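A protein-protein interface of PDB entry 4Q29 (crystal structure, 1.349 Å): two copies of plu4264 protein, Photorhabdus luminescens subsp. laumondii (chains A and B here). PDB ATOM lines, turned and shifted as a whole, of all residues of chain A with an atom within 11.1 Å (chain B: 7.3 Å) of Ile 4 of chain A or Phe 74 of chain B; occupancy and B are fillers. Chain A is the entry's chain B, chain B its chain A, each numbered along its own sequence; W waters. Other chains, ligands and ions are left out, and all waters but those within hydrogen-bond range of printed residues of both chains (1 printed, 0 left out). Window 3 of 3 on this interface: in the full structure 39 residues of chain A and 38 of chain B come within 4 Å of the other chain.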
ATOM      1  N   MET A   2       5.315  20.309 -18.591  1.00  0.00           N
ATOM      2  CA  MET A   2       6.601  19.846 -18.174  1.00  0.00           C
ATOM      3  C   MET A   2       6.505  18.346 -17.785  1.00  0.00           C
ATOM      4  O   MET A   2       5.498  17.889 -17.218  1.00  0.00           O
ATOM      5  CB  MET A   2       7.191  20.751 -17.067  1.00  0.00           C
ATOM      6  CG  MET A   2       8.443  20.125 -16.413  1.00  0.00           C
ATOM      7  SD  MET A   2       9.591  21.224 -15.307  1.00  0.00           S
ATOM      8  CE  MET A   2      10.923  20.001 -14.782  1.00  0.00           C
ATOM      9  N   ASN A   3       7.543  17.598 -18.155  1.00  0.00           N
ATOM     10  CA  ASN A   3       7.586  16.148 -18.009  1.00  0.00           C
ATOM     11  C   ASN A   3       8.382  15.791 -16.780  1.00  0.00           C
ATOM     12  O   ASN A   3       9.561  16.063 -16.690  1.00  0.00           O
ATOM     13  CB  ASN A   3       8.258  15.558 -19.241  1.00  0.00           C
ATOM     14  CG  ASN A   3       7.523  14.380 -19.795  1.00  0.00           C
ATOM     15  OD1 ASN A   3       8.122  13.339 -20.054  1.00  0.00           O
ATOM     16  ND2 ASN A   3       6.222  14.498 -19.923  1.00  0.00           N
ATOM     17  N   ILE A   4       7.664  15.218 -15.813  1.00  0.00           N
ATOM     18  CA  ILE A   4       8.188  14.651 -14.565  1.00  0.00           C
ATOM     19  C   ILE A   4       9.079  13.416 -14.768  1.00  0.00           C
ATOM     20  O   ILE A   4      10.118  13.281 -14.155  1.00  0.00           O
ATOM     21  CB  ILE A   4       6.982  14.290 -13.622  1.00  0.00           C
ATOM     22  CG1 ILE A   4       6.302  15.578 -13.158  1.00  0.00           C
ATOM     23  CG2 ILE A   4       7.399  13.397 -12.432  1.00  0.00           C
ATOM     24  CD1 ILE A   4       5.043  15.350 -12.376  1.00  0.00           C
ATOM     25  N   ILE A   5       8.653  12.508 -15.630  1.00  0.00           N
ATOM     26  CA  ILE A   5       9.290  11.172 -15.773  1.00  0.00           C
ATOM     27  C   ILE A   5       9.807  10.934 -17.159  1.00  0.00           C
ATOM     28  O   ILE A   5       9.155  11.267 -18.151  1.00  0.00           O
ATOM     29  CB  ILE A   5       8.361   9.984 -15.362  1.00  0.00           C
ATOM     30  CG1 ILE A   5       9.129   8.643 -15.423  1.00  0.00           C
ATOM     31  CG2 ILE A   5       7.108   9.932 -16.242  1.00  0.00           C
ATOM     32  CD1 ILE A   5       8.574   7.459 -14.560  1.00  0.00           C
ATOM     33  N   ARG A   6      10.986  10.342 -17.226  1.00  0.00           N
ATOM     34  CA  ARG A   6      11.487   9.764 -18.456  1.00  0.00           C
ATOM     35  C   ARG A   6      11.757   8.281 -18.202  1.00  0.00           C
ATOM     36  O   ARG A   6      12.729   7.922 -17.537  1.00  0.00           O
ATOM     37  CB  ARG A   6      12.764  10.439 -18.940  1.00  0.00           C
ATOM     38  CG  ARG A   6      13.256   9.837 -20.266  1.00  0.00           C
ATOM     39  CD  ARG A   6      14.671  10.257 -20.631  1.00  0.00           C
ATOM     40  NE  ARG A   6      14.781  11.665 -20.949  1.00  0.00           N
ATOM     41  CZ  ARG A   6      15.930  12.355 -20.898  1.00  0.00           C
ATOM     42  NH1 ARG A   6      15.934  13.591 -21.263  1.00  0.00           N
ATOM     43  NH2 ARG A   6      17.072  11.796 -20.536  1.00  0.00           N
ATOM     44  N   LYS A   7      10.910   7.453 -18.785  1.00  0.00           N
ATOM     45  CA  LYS A   7      11.117   5.995 -18.799  1.00  0.00           C
ATOM     46  C   LYS A   7      12.346   5.696 -19.606  1.00  0.00           C
ATOM     47  O   LYS A   7      12.512   6.141 -20.752  1.00  0.00           O
ATOM     48  CB  LYS A   7       9.903   5.242 -19.384  1.00  0.00           C
ATOM     49  CG  LYS A   7       8.568   5.383 -18.596  1.00  0.00           C
ATOM     50  CD  LYS A   7       7.724   4.076 -18.603  1.00  0.00           C
ATOM     51  CE  LYS A   7       8.209   3.058 -17.540  1.00  0.00           C
ATOM     52  NZ  LYS A   7       7.338   1.837 -17.466  1.00  0.00           N
ATOM     53  N   MET A   8      13.238   4.893 -19.040  1.00  0.00           N
ATOM     54  CA  MET A   8      14.421   4.511 -19.790  1.00  0.00           C
ATOM     55  C   MET A   8      14.063   3.659 -20.996  1.00  0.00           C
ATOM     56  O   MET A   8      13.387   2.632 -20.850  1.00  0.00           O
ATOM     57  CB  MET A   8      15.424   3.748 -18.915  1.00  0.00           C
ATOM     58  CG  MET A   8      16.480   3.036 -19.701  1.00  0.00           C
ATOM     59  SD  MET A   8      17.671   4.351 -20.573  1.00  0.00           S
ATOM     60  CE  MET A   8      18.886   4.535 -18.978  1.00  0.00           C
ATOM     61  N   LEU A  24      21.206  12.782 -19.952  1.00  0.00           N
ATOM     62  CA  LEU A  24      20.141  13.473 -19.240  1.00  0.00           C
ATOM     63  C   LEU A  24      19.518  14.610 -20.050  1.00  0.00           C
ATOM     64  O   LEU A  24      18.315  14.764 -20.100  1.00  0.00           O
ATOM     65  CB  LEU A  24      20.722  14.004 -17.932  1.00  0.00           C
ATOM     66  CG  LEU A  24      19.778  14.877 -17.123  1.00  0.00           C
ATOM     67  CD1 LEU A  24      18.553  14.107 -16.697  1.00  0.00           C
ATOM     68  CD2 LEU A  24      20.526  15.463 -15.929  1.00  0.00           C
ATOM     69  N   TRP A  27      16.361  18.062 -21.752  1.00  0.00           N
ATOM     70  CA  TRP A  27      15.110  17.737 -21.078  1.00  0.00           C
ATOM     71  C   TRP A  27      14.378  19.055 -20.916  1.00  0.00           C
ATOM     72  O   TRP A  27      14.735  19.843 -20.056  1.00  0.00           O
ATOM     73  CB  TRP A  27      15.419  17.076 -19.737  1.00  0.00           C
ATOM     74  CG  TRP A  27      14.220  16.516 -18.998  1.00  0.00           C
ATOM     75  CD1 TRP A  27      12.962  17.033 -18.937  1.00  0.00           C
ATOM     76  CD2 TRP A  27      14.196  15.310 -18.233  1.00  0.00           C
ATOM     77  NE1 TRP A  27      12.149  16.223 -18.155  1.00  0.00           N
ATOM     78  CE2 TRP A  27      12.901  15.172 -17.710  1.00  0.00           C
ATOM     79  CE3 TRP A  27      15.166  14.362 -17.915  1.00  0.00           C
ATOM     80  CZ2 TRP A  27      12.535  14.064 -16.929  1.00  0.00           C
ATOM     81  CZ3 TRP A  27      14.823  13.297 -17.110  1.00  0.00           C
ATOM     82  CH2 TRP A  27      13.521  13.166 -16.605  1.00  0.00           C
ATOM     83  N   GLU A  28      13.340  19.293 -21.705  1.00  0.00           N
ATOM     84  CA  GLU A  28      12.683  20.599 -21.616  1.00  0.00           C
ATOM     85  C   GLU A  28      12.072  20.826 -20.242  1.00  0.00           C
ATOM     86  O   GLU A  28      11.439  19.936 -19.690  1.00  0.00           O
ATOM     87  CB  GLU A  28      11.590  20.779 -22.663  1.00  0.00           C
ATOM     88  CG  GLU A  28      10.946  22.173 -22.648  1.00  0.00           C
ATOM     89  CD  GLU A  28      11.475  23.050 -23.758  1.00  0.00           C
ATOM     90  OE1 GLU A  28      10.810  24.056 -24.101  1.00  0.00           O
ATOM     91  OE2 GLU A  28      12.552  22.750 -24.307  1.00  0.00           O
ATOM     92  N   GLY A  29      12.249  22.038 -19.717  1.00  0.00           N
ATOM     93  CA  GLY A  29      11.737  22.400 -18.403  1.00  0.00           C
ATOM     94  C   GLY A  29      12.692  22.112 -17.258  1.00  0.00           C
ATOM     95  O   GLY A  29      12.460  22.547 -16.139  1.00  0.00           O
ATOM     96  N   LEU A  30      13.761  21.363 -17.524  1.00  0.00           N
ATOM     97  CA  LEU A  30      14.716  20.963 -16.487  1.00  0.00           C
ATOM     98  C   LEU A  30      15.950  21.857 -16.478  1.00  0.00           C
ATOM     99  O   LEU A  30      16.847  21.700 -17.298  1.00  0.00           O
ATOM    100  CB  LEU A  30      15.138  19.499 -16.663  1.00  0.00           C
ATOM    101  CG  LEU A  30      16.230  18.957 -15.739  1.00  0.00           C
ATOM    102  CD1 LEU A  30      15.753  19.011 -14.298  1.00  0.00           C
ATOM    103  CD2 LEU A  30      16.632  17.538 -16.190  1.00  0.00           C
ATOM    104  N   LEU B  57      16.178  15.472  -8.473  1.00  0.00           N
ATOM    105  CA  LEU B  57      16.079  14.454  -9.523  1.00  0.00           C
ATOM    106  C   LEU B  57      16.363  13.085  -8.897  1.00  0.00           C
ATOM    107  O   LEU B  57      17.297  12.949  -8.117  1.00  0.00           O
ATOM    108  CB  LEU B  57      17.101  14.709 -10.657  1.00  0.00           C
ATOM    109  CG  LEU B  57      17.168  13.848 -11.923  1.00  0.00           C
ATOM    110  CD1 LEU B  57      15.941  14.069 -12.787  1.00  0.00           C
ATOM    111  CD2 LEU B  57      18.453  14.170 -12.697  1.00  0.00           C
ATOM    112  N   PHE B  58      15.572  12.076  -9.276  1.00  0.00           N
ATOM    113  CA  PHE B  58      15.853  10.692  -8.903  1.00  0.00           C
ATOM    114  C   PHE B  58      16.340   9.948 -10.143  1.00  0.00           C
ATOM    115  O   PHE B  58      15.727  10.017 -11.209  1.00  0.00           O
ATOM    116  CB  PHE B  58      14.611   9.917  -8.430  1.00  0.00           C
ATOM    117  CG  PHE B  58      13.967  10.383  -7.166  1.00  0.00           C
ATOM    118  CD1 PHE B  58      14.534  11.302  -6.303  1.00  0.00           C
ATOM    119  CD2 PHE B  58      12.734   9.829  -6.839  1.00  0.00           C
ATOM    120  CE1 PHE B  58      13.895  11.653  -5.147  1.00  0.00           C
ATOM    121  CE2 PHE B  58      12.105  10.148  -5.694  1.00  0.00           C
ATOM    122  CZ  PHE B  58      12.663  11.045  -4.841  1.00  0.00           C
ATOM    123  N   ALA B  65       9.251   0.196  -8.036  1.00  0.00           N
ATOM    124  CA  ALA B  65       8.548   0.945  -6.966  1.00  0.00           C
ATOM    125  C   ALA B  65       7.706   2.165  -7.417  1.00  0.00           C
ATOM    126  O   ALA B  65       7.848   2.616  -8.544  1.00  0.00           O
ATOM    127  CB  ALA B  65       9.512   1.317  -5.846  1.00  0.00           C
ATOM    128  N   ILE B  66       6.869   2.739  -6.542  1.00  0.00           N
ATOM    129  CA  ILE B  66       5.963   3.832  -6.970  1.00  0.00           C
ATOM    130  C   ILE B  66       6.416   5.143  -6.380  1.00  0.00           C
ATOM    131  O   ILE B  66       6.647   5.237  -5.190  1.00  0.00           O
ATOM    132  CB  ILE B  66       4.499   3.468  -6.647  1.00  0.00           C
ATOM    133  CG1 ILE B  66       4.112   2.235  -7.464  1.00  0.00           C
ATOM    134  CG2 ILE B  66       3.598   4.599  -6.980  1.00  0.00           C
ATOM    135  CD1 ILE B  66       2.776   1.653  -7.204  1.00  0.00           C
ATOM    136  N   ILE B  67       6.598   6.150  -7.231  1.00  0.00           N
ATOM    137  CA  ILE B  67       6.862   7.495  -6.727  1.00  0.00           C
ATOM    138  C   ILE B  67       5.517   8.194  -6.758  1.00  0.00           C
ATOM    139  O   ILE B  67       4.921   8.328  -7.818  1.00  0.00           O
ATOM    140  CB  ILE B  67       7.916   8.280  -7.540  1.00  0.00           C
ATOM    141  CG1 ILE B  67       9.103   7.390  -7.946  1.00  0.00           C
ATOM    142  CG2 ILE B  67       8.383   9.520  -6.771  1.00  0.00           C
ATOM    143  CD1 ILE B  67       9.910   6.848  -6.804  1.00  0.00           C
ATOM    144  N   ARG B  68       5.051   8.661  -5.608  1.00  0.00           N
ATOM    145  CA  ARG B  68       3.802   9.407  -5.525  1.00  0.00           C
ATOM    146  C   ARG B  68       4.205  10.851  -5.392  1.00  0.00           C
ATOM    147  O   ARG B  68       4.909  11.211  -4.474  1.00  0.00           O
ATOM    148  CB  ARG B  68       2.968   8.958  -4.326  1.00  0.00           C
ATOM    149  CG  ARG B  68       1.598   9.664  -4.239  1.00  0.00           C
ATOM    150  CD  ARG B  68       0.588   8.943  -3.333  1.00  0.00           C
ATOM    151  NE  ARG B  68      -0.010   7.731  -3.949  1.00  0.00           N
ATOM    152  CZ  ARG B  68      -1.142   7.124  -3.547  1.00  0.00           C
ATOM    153  NH1 ARG B  68      -1.820   7.569  -2.503  1.00  0.00           N
ATOM    154  NH2 ARG B  68      -1.594   6.039  -4.180  1.00  0.00           N
ATOM    155  N   ILE B  69       3.773  11.648  -6.357  1.00  0.00           N
ATOM    156  CA  ILE B  69       4.082  13.070  -6.423  1.00  0.00           C
ATOM    157  C   ILE B  69       2.745  13.799  -6.440  1.00  0.00           C
ATOM    158  O   ILE B  69       1.979  13.693  -7.395  1.00  0.00           O
ATOM    159  CB  ILE B  69       4.905  13.409  -7.677  1.00  0.00           C
ATOM    160  CG1 ILE B  69       6.183  12.577  -7.752  1.00  0.00           C
ATOM    161  CG2 ILE B  69       5.248  14.882  -7.682  1.00  0.00           C
ATOM    162  CD1 ILE B  69       7.004  12.814  -8.999  1.00  0.00           C
ATOM    163  N   ASN B  70       2.450  14.490  -5.347  1.00  0.00           N
ATOM    164  CA  ASN B  70       1.144  15.116  -5.168  1.00  0.00           C
ATOM    165  C   ASN B  70       0.024  14.153  -5.541  1.00  0.00           C
ATOM    166  O   ASN B  70      -0.902  14.472  -6.336  1.00  0.00           O
ATOM    167  CB  ASN B  70       1.047  16.419  -5.964  1.00  0.00           C
ATOM    168  CG  ASN B  70       2.095  17.431  -5.538  1.00  0.00           C
ATOM    169  OD1 ASN B  70       2.826  17.998  -6.352  1.00  0.00           O
ATOM    170  ND2 ASN B  70       2.184  17.634  -4.256  1.00  0.00           N
ATOM    171  N   ASP B  71       0.105  12.989  -4.923  1.00  0.00           N
ATOM    172  CA  ASP B  71      -0.925  11.925  -5.075  1.00  0.00           C
ATOM    173  C   ASP B  71      -1.031  11.109  -6.419  1.00  0.00           C
ATOM    174  O   ASP B  71      -1.540   9.966  -6.407  1.00  0.00           O
ATOM    175  CB  ASP B  71      -2.273  12.482  -4.621  1.00  0.00           C
ATOM    176  CG  ASP B  71      -2.242  12.875  -3.159  1.00  0.00           C
ATOM    177  OD1 ASP B  71      -1.229  12.532  -2.503  1.00  0.00           O
ATOM    178  OD2 ASP B  71      -3.195  13.503  -2.664  1.00  0.00           O
ATOM    179  N   GLU B  72      -0.569  11.676  -7.537  1.00  0.00           N
ATOM    180  CA  GLU B  72      -0.423  10.893  -8.766  1.00  0.00           C
ATOM    181  C   GLU B  72       0.780   9.970  -8.673  1.00  0.00           C
ATOM    182  O   GLU B  72       1.850  10.360  -8.226  1.00  0.00           O
ATOM    183  CB  GLU B  72      -0.261  11.789  -9.979  1.00  0.00           C
ATOM    184  CG  GLU B  72      -1.415  12.721 -10.199  1.00  0.00           C
ATOM    185  CD  GLU B  72      -1.162  13.678 -11.347  1.00  0.00           C
ATOM    186  OE1 GLU B  72      -0.896  13.213 -12.477  1.00  0.00           O
ATOM    187  OE2 GLU B  72      -1.216  14.904 -11.119  1.00  0.00           O
ATOM    188  N   ASP B  73       0.602   8.745  -9.136  1.00  0.00           N
ATOM    189  CA  ASP B  73       1.571   7.691  -8.893  1.00  0.00           C
ATOM    190  C   ASP B  73       2.375   7.400 -10.162  1.00  0.00           C
ATOM    191  O   ASP B  73       1.806   7.207 -11.227  1.00  0.00           O
ATOM    192  CB  ASP B  73       0.825   6.441  -8.395  1.00  0.00           C
ATOM    193  CG  ASP B  73      -0.129   6.753  -7.268  1.00  0.00           C
ATOM    194  OD1 ASP B  73       0.044   7.785  -6.576  1.00  0.00           O
ATOM    195  OD2 ASP B  73      -1.101   5.990  -7.112  1.00  0.00           O
ATOM    196  N   PHE B  74       3.694   7.353  -9.994  1.00  0.00           N
ATOM    197  CA  PHE B  74       4.659   7.139 -11.089  1.00  0.00           C
ATOM    198  C   PHE B  74       5.416   5.831 -10.794  1.00  0.00           C
ATOM    199  O   PHE B  74       6.398   5.830 -10.039  1.00  0.00           O
ATOM    200  CB  PHE B  74       5.607   8.350 -11.161  1.00  0.00           C
ATOM    201  CG  PHE B  74       4.933   9.607 -11.661  1.00  0.00           C
ATOM    202  CD1 PHE B  74       4.281  10.465 -10.774  1.00  0.00           C
ATOM    203  CD2 PHE B  74       4.899   9.918 -13.017  1.00  0.00           C
ATOM    204  CE1 PHE B  74       3.641  11.640 -11.237  1.00  0.00           C
ATOM    205  CE2 PHE B  74       4.271  11.071 -13.469  1.00  0.00           C
ATOM    206  CZ  PHE B  74       3.642  11.928 -12.586  1.00  0.00           C
ATOM    207  N   PRO B  75       4.947   4.714 -11.383  1.00  0.00           N
ATOM    208  CA  PRO B  75       5.672   3.441 -11.460  1.00  0.00           C
ATOM    209  C   PRO B  75       7.080   3.600 -12.066  1.00  0.00           C
ATOM    210  O   PRO B  75       7.268   4.298 -13.079  1.00  0.00           O
ATOM    211  CB  PRO B  75       4.762   2.615 -12.361  1.00  0.00           C
ATOM    212  CG  PRO B  75       3.375   3.157 -12.099  1.00  0.00           C
ATOM    213  CD  PRO B  75       3.572   4.604 -11.914  1.00  0.00           C
ATOM    214  N   VAL B  76       8.061   2.968 -11.446  1.00  0.00           N
ATOM    215  CA  VAL B  76       9.455   3.123 -11.887  1.00  0.00           C
ATOM    216  C   VAL B  76      10.316   1.901 -11.695  1.00  0.00           C
ATOM    217  O   VAL B  76      10.082   1.051 -10.805  1.00  0.00           O
ATOM    218  CB  VAL B  76      10.146   4.356 -11.243  1.00  0.00           C
ATOM    219  CG1 VAL B  76       9.493   5.659 -11.717  1.00  0.00           C
ATOM    220  CG2 VAL B  76      10.155   4.247  -9.745  1.00  0.00           C
ATOM    221  N   THR B  77      11.336   1.810 -12.543  1.00  0.00           N
ATOM    222  CA  THR B  77      12.253   0.665 -12.636  1.00  0.00           C
ATOM    223  C   THR B  77      13.684   1.176 -12.895  1.00  0.00           C
ATOM    224  O   THR B  77      13.876   2.352 -13.253  1.00  0.00           O
ATOM    225  CB  THR B  77      11.872  -0.462 -13.779  1.00  0.00           C
ATOM    226  OG1 THR B  77      13.070  -0.844 -14.399  1.00  0.00           O
ATOM    227  CG2 THR B  77      11.148   0.013 -14.947  1.00  0.00           C
ATOM    228  N   ASP B  80      14.909   4.614 -15.042  1.00  0.00           N
ATOM    229  CA  ASP B  80      13.981   5.726 -15.094  1.00  0.00           C
ATOM    230  C   ASP B  80      14.542   6.907 -14.314  1.00  0.00           C
ATOM    231  O   ASP B  80      15.264   6.775 -13.342  1.00  0.00           O
ATOM    232  CB  ASP B  80      12.622   5.347 -14.499  1.00  0.00           C
ATOM    233  CG  ASP B  80      11.907   4.254 -15.285  1.00  0.00           C
ATOM    234  OD1 ASP B  80      12.274   3.985 -16.437  1.00  0.00           O
ATOM    235  OD2 ASP B  80      10.953   3.690 -14.729  1.00  0.00           O
ATOM    236  N   LEU B  81      14.212   8.088 -14.828  1.00  0.00           N
ATOM    237  CA  LEU B  81      14.545   9.355 -14.184  1.00  0.00           C
ATOM    238  C   LEU B  81      13.275  10.100 -13.899  1.00  0.00           C
ATOM    239  O   LEU B  81      12.357  10.097 -14.703  1.00  0.00           O
ATOM    240  CB  LEU B  81      15.402  10.207 -15.095  1.00  0.00           C
ATOM    241  CG  LEU B  81      16.476   9.552 -15.940  1.00  0.00           C
ATOM    242  CD1 LEU B  81      16.857  10.434 -17.086  1.00  0.00           C
ATOM    243  CD2 LEU B  81      17.683   9.194 -15.106  1.00  0.00           C
ATOM    244  N   ILE B  82      13.254  10.743 -12.695  1.00  0.00           N
ATOM    245  CA  ILE B  82      12.122  11.444 -12.127  1.00  0.00           C
ATOM    246  C   ILE B  82      12.578  12.793 -11.647  1.00  0.00           C
ATOM    247  O   ILE B  82      13.499  12.884 -10.858  1.00  0.00           O
ATOM    248  CB  ILE B  82      11.565  10.656 -10.926  1.00  0.00           C
ATOM    249  CG1 ILE B  82      10.801   9.422 -11.418  1.00  0.00           C
ATOM    250  CG2 ILE B  82      10.758  11.559  -9.987  1.00  0.00           C
ATOM    251  CD1 ILE B  82       9.286   9.592 -11.620  1.00  0.00           C
ATOM    252  N   ILE B  83      11.903  13.823 -12.135  1.00  0.00           N
ATOM    253  CA  ILE B  83      12.079  15.164 -11.597  1.00  0.00           C
ATOM    254  C   ILE B  83      11.026  15.378 -10.539  1.00  0.00           C
ATOM    255  O   ILE B  83       9.859  15.037 -10.705  1.00  0.00           O
ATOM    256  CB  ILE B  83      11.961  16.263 -12.648  1.00  0.00           C
ATOM    257  CG1 ILE B  83      13.272  16.435 -13.376  1.00  0.00           C
ATOM    258  CG2 ILE B  83      11.656  17.623 -11.997  1.00  0.00           C
ATOM    259  CD1 ILE B  83      13.498  15.480 -14.397  1.00  0.00           C
ATOM    260  N   ILE B  84      11.447  15.930  -9.429  1.00  0.00           N
ATOM    261  CA  ILE B  84      10.488  16.314  -8.423  1.00  0.00           C
ATOM    262  C   ILE B  84      10.131  17.790  -8.625  1.00  0.00           C
ATOM    263  O   ILE B  84      10.978  18.687  -8.466  1.00  0.00           O
ATOM    264  CB  ILE B  84      11.047  16.142  -7.047  1.00  0.00           C
ATOM    265  CG1 ILE B  84      11.453  14.718  -6.761  1.00  0.00           C
ATOM    266  CG2 ILE B  84      10.021  16.631  -6.007  1.00  0.00           C
ATOM    267  CD1 ILE B  84      10.327  13.688  -6.940  1.00  0.00           C
ATOM    268  N   PRO B  85       8.877  18.075  -8.968  1.00  0.00           N
ATOM    269  CA  PRO B  85       8.550  19.502  -9.016  1.00  0.00           C
ATOM    270  C   PRO B  85       8.734  20.169  -7.666  1.00  0.00           C
ATOM    271  O   PRO B  85       8.579  19.650  -6.578  1.00  0.00           O
ATOM    272  CB  PRO B  85       7.087  19.489  -9.426  1.00  0.00           C
ATOM    273  CG  PRO B  85       6.947  18.229 -10.209  1.00  0.00           C
ATOM    274  CD  PRO B  85       7.750  17.252  -9.449  1.00  0.00           C
ATOM    275  N   SER B  88       6.654  20.019  -4.258  1.00  0.00           N
ATOM    276  CA  SER B  88       5.719  18.879  -4.357  1.00  0.00           C
ATOM    277  C   SER B  88       5.704  18.000  -3.103  1.00  0.00           C
ATOM    278  O   SER B  88       6.641  17.958  -2.359  1.00  0.00           O
ATOM    279  CB  SER B  88       5.974  18.007  -5.605  1.00  0.00           C
ATOM    280  OG  SER B  88       7.334  17.758  -5.908  1.00  0.00           O
HETATM  281  O   HOH W   1      12.435   1.687 -18.042  1.00  0.00           O
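OD1 of Asp 80 of chain B lies within hydrogen-bond range of N of Met 8 of chain A, at 2.9 Å. N of Arg 6 of chain A lies within hydrogen-bond range of O of Leu 81 of chain B (2.9 Å). N of Ile 83 of chain B is in hydrogen-bond range of O of Ile 4 of chain A, 2.7 Å away.
O of Ile 82 of chain B sits at hydrogen-bond distance from N of Phe 58 of chain B, 2.7 Å away. O of Ala 65 of chain B lies within hydrogen-bond range of N of Val 76 of chain B, 2.9 Å away. The backbone carbonyl oxygen of Ile 67 of chain B lies within hydrogen-bond range of the backbone NH of Phe 74 of chain B (2.7 Å). The backbone NH (N) of Thr 77 of chain B lies within hydrogen-bond range of the side-chain carboxylate (OD2) of Asp 80 of chain B (2.9 Å). The backbone carbonyl oxygen (O) of Ile 5 of chain A lies close to the side-chain amide oxygen (OD1) of Asn 3 of chain A. The guanidinium group (NH1) of Arg 6 of chain A sits at hydrogen-bond distance from the backbone carbonyl oxygen (O) of Leu 24 of chain A (2.9 Å).
Among the printed residues, merely in contact across the chains: Met 2 of chain A with Ile 83 of chain B, Ile 4 of chain A with Ile 69 of chain B, Ile 4 of chain A with Phe 74 of chain B, Ile 4 of chain A with Leu 81 of chain B, Ile 4 of chain A with Ile 82 of chain B, Ile 5 of chain A with Phe 74 of chain B, Ile 5 of chain A with Pro 75 of chain B, Ile 5 of chain A with Val 76 of chain B, Ile 5 of chain A with Leu 81 of chain B, Ile 5 of chain A with Ile 82 of chain B, Arg 6 of chain A with Asp 80 of chain B, Lys 7 of chain A with Asp 80 of chain B, Trp 27 of chain A with Leu 81 of chain B, Trp 27 of chain A with Ile 83 of chain B and Leu 30 of chain A with Ile 83 of chain B.
Of the printed residues of chain B, Ile 4 of chain A touches Ile 69, Phe 74, Leu 81, Ile 82 and Ile 83. No residue of chain A comes within 4 Å of Ala 65 of chain B. No residue of chain A comes within 4 Å of Ile 66 of chain B. No residue of chain A comes within 4 Å of Asp 73 of chain B. Of chain A, only Ile 5 comes within 4 Å of Pro 75 of chain B. Printed residues of chain B within 4 Å of Met 8 of chain A: Asp 80 (2.9 Å). Of the printed residues of chain B, Arg 6 of chain A touches Asp 80 and Leu 81.
Of the 12 printed residues of chain A, 8 touch a printed residue of chain B. Hydrophobic or aromatic side chains of chain A within 4 Å of the printed part of chain B: Met 2, Ile 4, Ile 5, Trp 27 and Leu 30. Along chain A the printed residues that touch a printed residue of chain B span positions 2 to 30. Of the 22 printed residues of chain B, 8 touch a printed residue of chain A. Among the printed residues, no Asp or Glu carboxylate lies within 4 Å of a Lys or Arg side-chain nitrogen of the other chain.
No position is printed for both chains.
Water W1 bridges the side-chain carboxylate (OD1) of Asp 80 of chain B (2.8 Å) and the backbone carbonyl oxygen (O) of Met 8 of chain A (3.1 Å).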
